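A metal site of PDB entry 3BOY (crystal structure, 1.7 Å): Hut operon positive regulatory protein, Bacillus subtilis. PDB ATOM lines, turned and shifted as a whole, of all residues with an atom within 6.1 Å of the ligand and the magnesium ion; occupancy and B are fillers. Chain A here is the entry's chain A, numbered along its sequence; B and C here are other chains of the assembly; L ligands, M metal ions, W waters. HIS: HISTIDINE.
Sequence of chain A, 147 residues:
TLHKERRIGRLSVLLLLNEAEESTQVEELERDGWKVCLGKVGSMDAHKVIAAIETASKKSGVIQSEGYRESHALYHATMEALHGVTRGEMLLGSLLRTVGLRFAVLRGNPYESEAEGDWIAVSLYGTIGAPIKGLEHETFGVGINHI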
ATOM      1  N   TYR A  68       7.806  38.947  30.256  1.00  0.00           N
ATOM      2  CA  TYR A  68       7.900  37.703  29.478  1.00  0.00           C
ATOM      3  C   TYR A  68       6.540  37.088  29.162  1.00  0.00           C
ATOM      4  O   TYR A  68       6.340  36.611  28.045  1.00  0.00           O
ATOM      5  CB  TYR A  68       8.725  36.676  30.224  1.00  0.00           C
ATOM      6  CG  TYR A  68       9.077  35.444  29.418  1.00  0.00           C
ATOM      7  CD1 TYR A  68       9.399  35.541  28.037  1.00  0.00           C
ATOM      8  CD2 TYR A  68       9.124  34.203  30.037  1.00  0.00           C
ATOM      9  CE1 TYR A  68       9.748  34.351  27.273  1.00  0.00           C
ATOM     10  CE2 TYR A  68       9.473  33.027  29.292  1.00  0.00           C
ATOM     11  CZ  TYR A  68       9.804  33.125  27.940  1.00  0.00           C
ATOM     12  OH  TYR A  68      10.163  31.965  27.244  1.00  0.00           O
ATOM     13  N   SER A  71       4.923  37.786  25.682  1.00  0.00           N
ATOM     14  CA  SER A  71       5.880  37.284  24.694  1.00  0.00           C
ATOM     15  C   SER A  71       5.884  35.749  24.661  1.00  0.00           C
ATOM     16  O   SER A  71       5.939  35.165  23.576  1.00  0.00           O
ATOM     17  CB  SER A  71       7.291  37.795  25.031  1.00  0.00           C
ATOM     18  OG  SER A  71       7.312  39.208  24.864  1.00  0.00           O
ATOM     19  N   HIS A  72       5.794  35.119  25.832  1.00  0.00           N
ATOM     20  CA  HIS A  72       5.777  33.653  25.896  1.00  0.00           C
ATOM     21  C   HIS A  72       4.528  33.131  25.186  1.00  0.00           C
ATOM     22  O   HIS A  72       4.608  32.212  24.363  1.00  0.00           O
ATOM     23  CB  HIS A  72       5.777  33.154  27.337  1.00  0.00           C
ATOM     24  CG  HIS A  72       5.933  31.670  27.443  1.00  0.00           C
ATOM     25  ND1 HIS A  72       4.893  30.834  27.775  1.00  0.00           N
ATOM     26  CD2 HIS A  72       7.019  30.882  27.290  1.00  0.00           C
ATOM     27  CE1 HIS A  72       5.320  29.586  27.785  1.00  0.00           C
ATOM     28  NE2 HIS A  72       6.612  29.588  27.505  1.00  0.00           N
ATOM     29  N   TYR A  75       4.919  33.642  21.416  1.00  0.00           N
ATOM     30  CA  TYR A  75       5.900  32.729  20.809  1.00  0.00           C
ATOM     31  C   TYR A  75       5.244  31.347  20.520  1.00  0.00           C
ATOM     32  O   TYR A  75       5.346  30.789  19.440  1.00  0.00           O
ATOM     33  CB  TYR A  75       7.081  32.523  21.758  1.00  0.00           C
ATOM     34  CG  TYR A  75       8.174  31.684  21.145  1.00  0.00           C
ATOM     35  CD1 TYR A  75       9.061  32.228  20.174  1.00  0.00           C
ATOM     36  CD2 TYR A  75       8.302  30.327  21.472  1.00  0.00           C
ATOM     37  CE1 TYR A  75      10.079  31.426  19.602  1.00  0.00           C
ATOM     38  CE2 TYR A  75       9.271  29.527  20.926  1.00  0.00           C
ATOM     39  CZ  TYR A  75      10.192  30.074  19.987  1.00  0.00           C
ATOM     40  OH  TYR A  75      11.212  29.295  19.424  1.00  0.00           O
ATOM     41  N   HIS A  76       4.537  30.843  21.506  1.00  0.00           N
ATOM     42  CA  HIS A  76       3.969  29.503  21.344  1.00  0.00           C
ATOM     43  C   HIS A  76       2.817  29.508  20.377  1.00  0.00           C
ATOM     44  O   HIS A  76       2.684  28.572  19.589  1.00  0.00           O
ATOM     45  CB  HIS A  76       3.590  28.961  22.673  1.00  0.00           C
ATOM     46  CG  HIS A  76       4.751  28.401  23.427  1.00  0.00           C
ATOM     47  ND1 HIS A  76       5.279  27.158  23.144  1.00  0.00           N
ATOM     48  CD2 HIS A  76       5.516  28.935  24.410  1.00  0.00           C
ATOM     49  CE1 HIS A  76       6.284  26.914  23.971  1.00  0.00           C
ATOM     50  NE2 HIS A  76       6.460  27.991  24.727  1.00  0.00           N
ATOM     51  N   VAL B  85      14.622  19.201  26.332  1.00  0.00           N
ATOM     52  CA  VAL B  85      14.985  20.596  26.281  1.00  0.00           C
ATOM     53  C   VAL B  85      14.230  21.360  25.193  1.00  0.00           C
ATOM     54  O   VAL B  85      13.746  22.453  25.470  1.00  0.00           O
ATOM     55  CB  VAL B  85      16.535  20.768  26.123  1.00  0.00           C
ATOM     56  CG1 VAL B  85      16.924  22.245  25.914  1.00  0.00           C
ATOM     57  CG2 VAL B  85      17.252  20.185  27.349  1.00  0.00           C
ATOM     58  N   THR B  86      14.102  20.765  23.998  1.00  0.00           N
ATOM     59  CA  THR B  86      13.561  21.460  22.817  1.00  0.00           C
ATOM     60  C   THR B  86      12.061  21.205  22.556  1.00  0.00           C
ATOM     61  O   THR B  86      11.407  21.990  21.876  1.00  0.00           O
ATOM     62  CB  THR B  86      14.369  21.154  21.550  1.00  0.00           C
ATOM     63  OG1 THR B  86      14.402  19.753  21.291  1.00  0.00           O
ATOM     64  CG2 THR B  86      15.824  21.657  21.696  1.00  0.00           C
ATOM     65  N   ARG B  87      11.571  20.095  23.070  1.00  0.00           N
ATOM     66  CA  ARG B  87      10.103  19.843  23.082  1.00  0.00           C
ATOM     67  C   ARG B  87       9.427  19.965  21.690  1.00  0.00           C
ATOM     68  O   ARG B  87       8.369  20.601  21.540  1.00  0.00           O
ATOM     69  CB  ARG B  87       9.432  20.663  24.174  1.00  0.00           C
ATOM     70  CG  ARG B  87       9.781  20.174  25.592  1.00  0.00           C
ATOM     71  CD  ARG B  87       9.815  21.339  26.586  1.00  0.00           C
ATOM     72  NE  ARG B  87      10.851  22.330  26.195  1.00  0.00           N
ATOM     73  CZ  ARG B  87      10.623  23.595  25.861  1.00  0.00           C
ATOM     74  NH1 ARG B  87       9.379  24.110  25.847  1.00  0.00           N
ATOM     75  NH2 ARG B  87      11.646  24.351  25.476  1.00  0.00           N
ATOM     76  N   LEU B  95      14.866  29.054  15.503  1.00  0.00           N
ATOM     77  CA  LEU B  95      13.546  29.384  15.994  1.00  0.00           C
ATOM     78  C   LEU B  95      13.605  30.530  16.992  1.00  0.00           C
ATOM     79  O   LEU B  95      12.754  30.645  17.885  1.00  0.00           O
ATOM     80  CB  LEU B  95      12.893  28.138  16.669  1.00  0.00           C
ATOM     81  CG  LEU B  95      12.692  26.915  15.771  1.00  0.00           C
ATOM     82  CD1 LEU B  95      11.921  25.928  16.657  1.00  0.00           C
ATOM     83  CD2 LEU B  95      11.902  27.267  14.496  1.00  0.00           C
ATOM     84  N   LEU B  96      14.629  31.393  16.842  1.00  0.00           N
ATOM     85  CA  LEU B  96      14.743  32.600  17.694  1.00  0.00           C
ATOM     86  C   LEU B  96      14.747  32.265  19.209  1.00  0.00           C
ATOM     87  O   LEU B  96      14.169  32.980  20.038  1.00  0.00           O
ATOM     88  CB  LEU B  96      13.679  33.645  17.314  1.00  0.00           C
ATOM     89  CG  LEU B  96      14.014  35.132  17.539  1.00  0.00           C
ATOM     90  CD1 LEU B  96      15.305  35.568  16.807  1.00  0.00           C
ATOM     91  CD2 LEU B  96      12.861  36.003  17.080  1.00  0.00           C
ATOM     92  N   ARG B  97      15.453  31.194  19.564  1.00  0.00           N
ATOM     93  CA  ARG B  97      15.677  30.916  20.966  1.00  0.00           C
ATOM     94  C   ARG B  97      17.104  30.495  21.317  1.00  0.00           C
ATOM     95  O   ARG B  97      17.885  30.022  20.465  1.00  0.00           O
ATOM     96  CB  ARG B  97      14.626  29.911  21.488  1.00  0.00           C
ATOM     97  CG  ARG B  97      14.705  28.533  20.911  1.00  0.00           C
ATOM     98  CD  ARG B  97      13.576  27.598  21.526  1.00  0.00           C
ATOM     99  NE  ARG B  97      13.634  26.327  20.824  1.00  0.00           N
ATOM    100  CZ  ARG B  97      12.793  25.312  21.021  1.00  0.00           C
ATOM    101  NH1 ARG B  97      11.836  25.390  21.958  1.00  0.00           N
ATOM    102  NH2 ARG B  97      12.940  24.225  20.260  1.00  0.00           N
ATOM    103  N   THR B  98      17.448  30.669  22.585  1.00  0.00           N
ATOM    104  CA  THR B  98      18.800  30.386  23.056  1.00  0.00           C
ATOM    105  C   THR B  98      18.659  29.554  24.327  1.00  0.00           C
ATOM    106  O   THR B  98      17.646  29.687  25.017  1.00  0.00           O
ATOM    107  CB  THR B  98      19.511  31.773  23.370  1.00  0.00           C
ATOM    108  OG1 THR B  98      20.775  31.513  24.014  1.00  0.00           O
ATOM    109  CG2 THR B  98      18.653  32.646  24.277  1.00  0.00           C
ATOM    110  N   ILE B 128      15.758  28.357  28.671  1.00  0.00           N
ATOM    111  CA  ILE B 128      15.593  28.518  27.226  1.00  0.00           C
ATOM    112  C   ILE B 128      14.713  29.749  27.083  1.00  0.00           C
ATOM    113  O   ILE B 128      13.810  29.985  27.922  1.00  0.00           O
ATOM    114  CB  ILE B 128      14.956  27.225  26.622  1.00  0.00           C
ATOM    115  CG1 ILE B 128      14.955  27.250  25.092  1.00  0.00           C
ATOM    116  CG2 ILE B 128      13.604  26.984  27.268  1.00  0.00           C
ATOM    117  CD1 ILE B 128      14.670  25.878  24.458  1.00  0.00           C
ATOM    118  N   GLY B 129      14.970  30.572  26.080  1.00  0.00           N
ATOM    119  CA  GLY B 129      14.217  31.804  25.982  1.00  0.00           C
ATOM    120  C   GLY B 129      14.485  32.557  24.728  1.00  0.00           C
ATOM    121  O   GLY B 129      15.273  32.093  23.884  1.00  0.00           O
ATOM    122  N   ALA B 130      13.844  33.706  24.600  1.00  0.00           N
ATOM    123  CA  ALA B 130      14.187  34.681  23.542  1.00  0.00           C
ATOM    124  C   ALA B 130      15.623  35.152  23.831  1.00  0.00           C
ATOM    125  O   ALA B 130      16.051  35.017  24.964  1.00  0.00           O
ATOM    126  CB  ALA B 130      13.231  35.841  23.562  1.00  0.00           C
ATOM    127  N   PRO B 131      16.356  35.630  22.817  1.00  0.00           N
ATOM    128  CA  PRO B 131      17.702  36.157  23.099  1.00  0.00           C
ATOM    129  C   PRO B 131      17.731  37.515  23.813  1.00  0.00           C
ATOM    130  O   PRO B 131      18.450  38.420  23.397  1.00  0.00           O
ATOM    131  CB  PRO B 131      18.334  36.270  21.706  1.00  0.00           C
ATOM    132  CG  PRO B 131      17.193  36.462  20.767  1.00  0.00           C
ATOM    133  CD  PRO B 131      16.024  35.694  21.376  1.00  0.00           C
ATOM    134  N   LEU B 135      13.847  36.958  29.438  1.00  0.00           N
ATOM    135  CA  LEU B 135      12.723  36.469  28.636  1.00  0.00           C
ATOM    136  C   LEU B 135      12.935  34.988  28.452  1.00  0.00           C
ATOM    137  O   LEU B 135      13.228  34.523  27.341  1.00  0.00           O
ATOM    138  CB  LEU B 135      12.663  37.182  27.286  1.00  0.00           C
ATOM    139  CG  LEU B 135      12.292  38.682  27.276  1.00  0.00           C
ATOM    140  CD1 LEU B 135      11.773  39.085  25.915  1.00  0.00           C
ATOM    141  CD2 LEU B 135      11.277  39.011  28.332  1.00  0.00           C
ATOM    142  N   GLU B 136      12.806  34.249  29.537  1.00  0.00           N
ATOM    143  CA  GLU B 136      13.212  32.824  29.553  1.00  0.00           C
ATOM    144  C   GLU B 136      12.490  32.071  30.642  1.00  0.00           C
ATOM    145  O   GLU B 136      11.988  32.679  31.589  1.00  0.00           O
ATOM    146  CB  GLU B 136      14.728  32.720  29.797  1.00  0.00           C
ATOM    147  CG  GLU B 136      15.181  33.286  31.188  1.00  0.00           C
ATOM    148  CD  GLU B 136      16.627  33.771  31.211  1.00  0.00           C
ATOM    149  OE1 GLU B 136      17.040  34.440  30.243  1.00  0.00           O
ATOM    150  OE2 GLU B 136      17.336  33.467  32.205  1.00  0.00           O
ATOM    151  N   HIS B 137      12.408  30.755  30.476  1.00  0.00           N
ATOM    152  CA  HIS B 137      12.008  29.849  31.548  1.00  0.00           C
ATOM    153  C   HIS B 137      12.911  28.639  31.620  1.00  0.00           C
ATOM    154  O   HIS B 137      13.780  28.467  30.757  1.00  0.00           O
ATOM    155  CB  HIS B 137      10.487  29.460  31.469  1.00  0.00           C
ATOM    156  CG  HIS B 137      10.096  28.718  30.215  1.00  0.00           C
ATOM    157  ND1 HIS B 137      10.581  27.454  29.895  1.00  0.00           N
ATOM    158  CD2 HIS B 137       9.228  29.043  29.227  1.00  0.00           C
ATOM    159  CE1 HIS B 137      10.070  27.062  28.742  1.00  0.00           C
ATOM    160  NE2 HIS B 137       9.241  28.005  28.316  1.00  0.00           N
ATOM    161  N   GLU C  80       4.297  19.222  26.964  1.00  0.00           N
ATOM    162  CA  GLU C  80       5.743  19.518  26.966  1.00  0.00           C
ATOM    163  C   GLU C  80       6.522  18.525  27.860  1.00  0.00           C
ATOM    164  O   GLU C  80       7.581  18.015  27.491  1.00  0.00           O
ATOM    165  CB  GLU C  80       5.998  20.999  27.279  1.00  0.00           C
ATOM    166  CG  GLU C  80       5.425  21.950  26.178  1.00  0.00           C
ATOM    167  CD  GLU C  80       5.985  23.406  26.169  1.00  0.00           C
ATOM    168  OE1 GLU C  80       6.920  23.633  26.917  1.00  0.00           O
ATOM    169  N   TRP C 119       2.652  30.810  36.859  1.00  0.00           N
ATOM    170  CA  TRP C 119       3.132  29.832  35.864  1.00  0.00           C
ATOM    171  C   TRP C 119       2.938  28.452  36.449  1.00  0.00           C
ATOM    172  O   TRP C 119       2.728  28.290  37.653  1.00  0.00           O
ATOM    173  CB  TRP C 119       4.615  30.071  35.566  1.00  0.00           C
ATOM    174  CG  TRP C 119       4.836  31.357  34.821  1.00  0.00           C
ATOM    175  CD1 TRP C 119       4.579  32.628  35.260  1.00  0.00           C
ATOM    176  CD2 TRP C 119       5.341  31.491  33.508  1.00  0.00           C
ATOM    177  NE1 TRP C 119       4.871  33.531  34.295  1.00  0.00           N
ATOM    178  CE2 TRP C 119       5.359  32.859  33.198  1.00  0.00           C
ATOM    179  CE3 TRP C 119       5.786  30.566  32.542  1.00  0.00           C
ATOM    180  CZ2 TRP C 119       5.799  33.350  31.968  1.00  0.00           C
ATOM    181  CZ3 TRP C 119       6.226  31.048  31.324  1.00  0.00           C
ATOM    182  CH2 TRP C 119       6.231  32.425  31.038  1.00  0.00           C
ATOM    183  N   ILE C 144       6.766  23.609  31.196  1.00  0.00           N
ATOM    184  CA  ILE C 144       6.479  24.856  31.928  1.00  0.00           C
ATOM    185  C   ILE C 144       5.615  25.760  31.075  1.00  0.00           C
ATOM    186  O   ILE C 144       5.856  25.934  29.882  1.00  0.00           O
ATOM    187  CB  ILE C 144       7.830  25.522  32.327  1.00  0.00           C
ATOM    188  CG1 ILE C 144       8.443  24.688  33.504  1.00  0.00           C
ATOM    189  CG2 ILE C 144       7.656  26.952  32.805  1.00  0.00           C
ATOM    190  CD1 ILE C 144       9.925  24.852  33.765  1.00  0.00           C
ATOM    191  N   ASN C 145       4.560  26.326  31.650  1.00  0.00           N
ATOM    192  CA  ASN C 145       3.696  27.215  30.902  1.00  0.00           C
ATOM    193  C   ASN C 145       3.186  28.397  31.748  1.00  0.00           C
ATOM    194  O   ASN C 145       3.176  28.290  32.971  1.00  0.00           O
ATOM    195  CB  ASN C 145       2.502  26.407  30.358  1.00  0.00           C
ATOM    196  CG  ASN C 145       1.886  27.015  29.131  1.00  0.00           C
ATOM    197  OD1 ASN C 145       2.386  27.989  28.549  1.00  0.00           O
ATOM    198  ND2 ASN C 145       0.777  26.432  28.696  1.00  0.00           N
HETATM  199  CA  HIS L   1       9.998  29.036  24.615  1.00  0.00           C
HETATM  200  C   HIS L   1      10.192  27.539  24.794  1.00  0.00           C
HETATM  201  O   HIS L   1       9.349  26.977  25.512  1.00  0.00           O
HETATM  202  CB  HIS L   1      11.338  29.792  24.510  1.00  0.00           C
HETATM  203  CG  HIS L   1      11.175  31.166  23.952  1.00  0.00           C
HETATM  204  ND1 HIS L   1      10.633  32.207  24.668  1.00  0.00           N
HETATM  205  CD2 HIS L   1      11.486  31.667  22.730  1.00  0.00           C
HETATM  206  CE1 HIS L   1      10.571  33.285  23.896  1.00  0.00           C
HETATM  207  NE2 HIS L   1      11.079  32.984  22.720  1.00  0.00           N
HETATM  208  OXT HIS L   1      11.091  26.901  24.261  1.00  0.00           O
HETATM  209 MG    MG M   1       7.895  28.011  26.539  1.00  0.00          MG
HETATM  210  O   HOH W   1       9.869  36.352  22.499  1.00  0.00           O
HETATM  211  O   HOH W   2       6.836  26.391  27.328  1.00  0.00           O
HETATM  212  O   HOH W   3      12.128  34.629  20.687  1.00  0.00           O
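Merely in contact with the ligand: Tyr 75, Ile 128 of chain B and Gly 129 of chain B.
Hydrophobic or aromatic side chains that line the ligand: Tyr 68, Tyr 75, His 76, Ile 128 of chain B, Ala 130 of chain B and His 137 of chain B.
Nine residues have an atom within 4 Å of the ligand: Tyr 68, Tyr 75, His 76, Arg 87 of chain B, Arg 97 of chain B, Ile 128 of chain B, Gly 129 of chain B, Ala 130 of chain B and His 137 of chain B.
Three residues have an atom within 4 Å of the magnesium ion: His 72, His 76 and His 137 of chain B.
Along chain A the residues within 4 Å of the magnesium ion span positions 72 to 76.
The nearest printed residue that does not touch the magnesium ion is Arg 87 of chain B (4.2 Å).
A nitrogen (ND1) of the ligand is in hydrogen-bond range of the side-chain hydroxyl (OH) of Tyr 68 (2.6 Å).
The guanidinium group of Arg 97 of chain B lies within salt-bridge range of an oxygen (OXT) of the ligand, at 2.9 Å.
NH2 of Arg 87 of chain B is in salt-bridge range of OXT of the ligand, at 2.9 Å.
NE2 of the ligand lies close to N of Ala 130 of chain B.
O of His 137 of chain B sits at hydrogen-bond distance from N of Ile 128 of chain B, at 2.9 Å.
O of Thr 86 of chain B is in hydrogen-bond range of NH2 of Arg 97 of chain B, at 3.2 Å.
The guanidinium group (NH1) of Arg 87 of chain B lies within salt-bridge range of the side-chain carboxylate (OE1) of Glu 80 of chain C.
The backbone carbonyl oxygen of Leu 95 of chain B sits at hydrogen-bond distance from the side-chain hydroxyl of Tyr 75, at 2.6 Å.
N of Ala 130 of chain B sits at hydrogen-bond distance from O of Leu 135 of chain B (2.9 Å).
The backbone NH (N) of Thr 98 of chain B lies within hydrogen-bond range of the backbone carbonyl oxygen (O) of Gly 129 of chain B (2.9 Å).
Water W2 lies within hydrogen-bond range of O of Ile 144 of chain C (2.8 Å) and OE1 of Glu 80 of chain C (2.8 Å).
Water W3 lies within hydrogen-bond range of the backbone carbonyl oxygen of Leu 96 of chain B and a nitrogen (NE2) of the ligand.
O of the ligand binds the magnesium ion (2.1 Å).
Water W2 is bound to the magnesium ion, 2.1 Å away.
A ring nitrogen (NE2) of His 137 of chain B is bound to the magnesium ion (2.2 Å).
A ring nitrogen (NE2) of His 72 binds the magnesium ion, 2.3 Å away.
The magnesium ion is bound by a ring nitrogen (NE2) of His 76, 2.3 Å away.
The magnesium ion has five donor atoms within binding distance.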
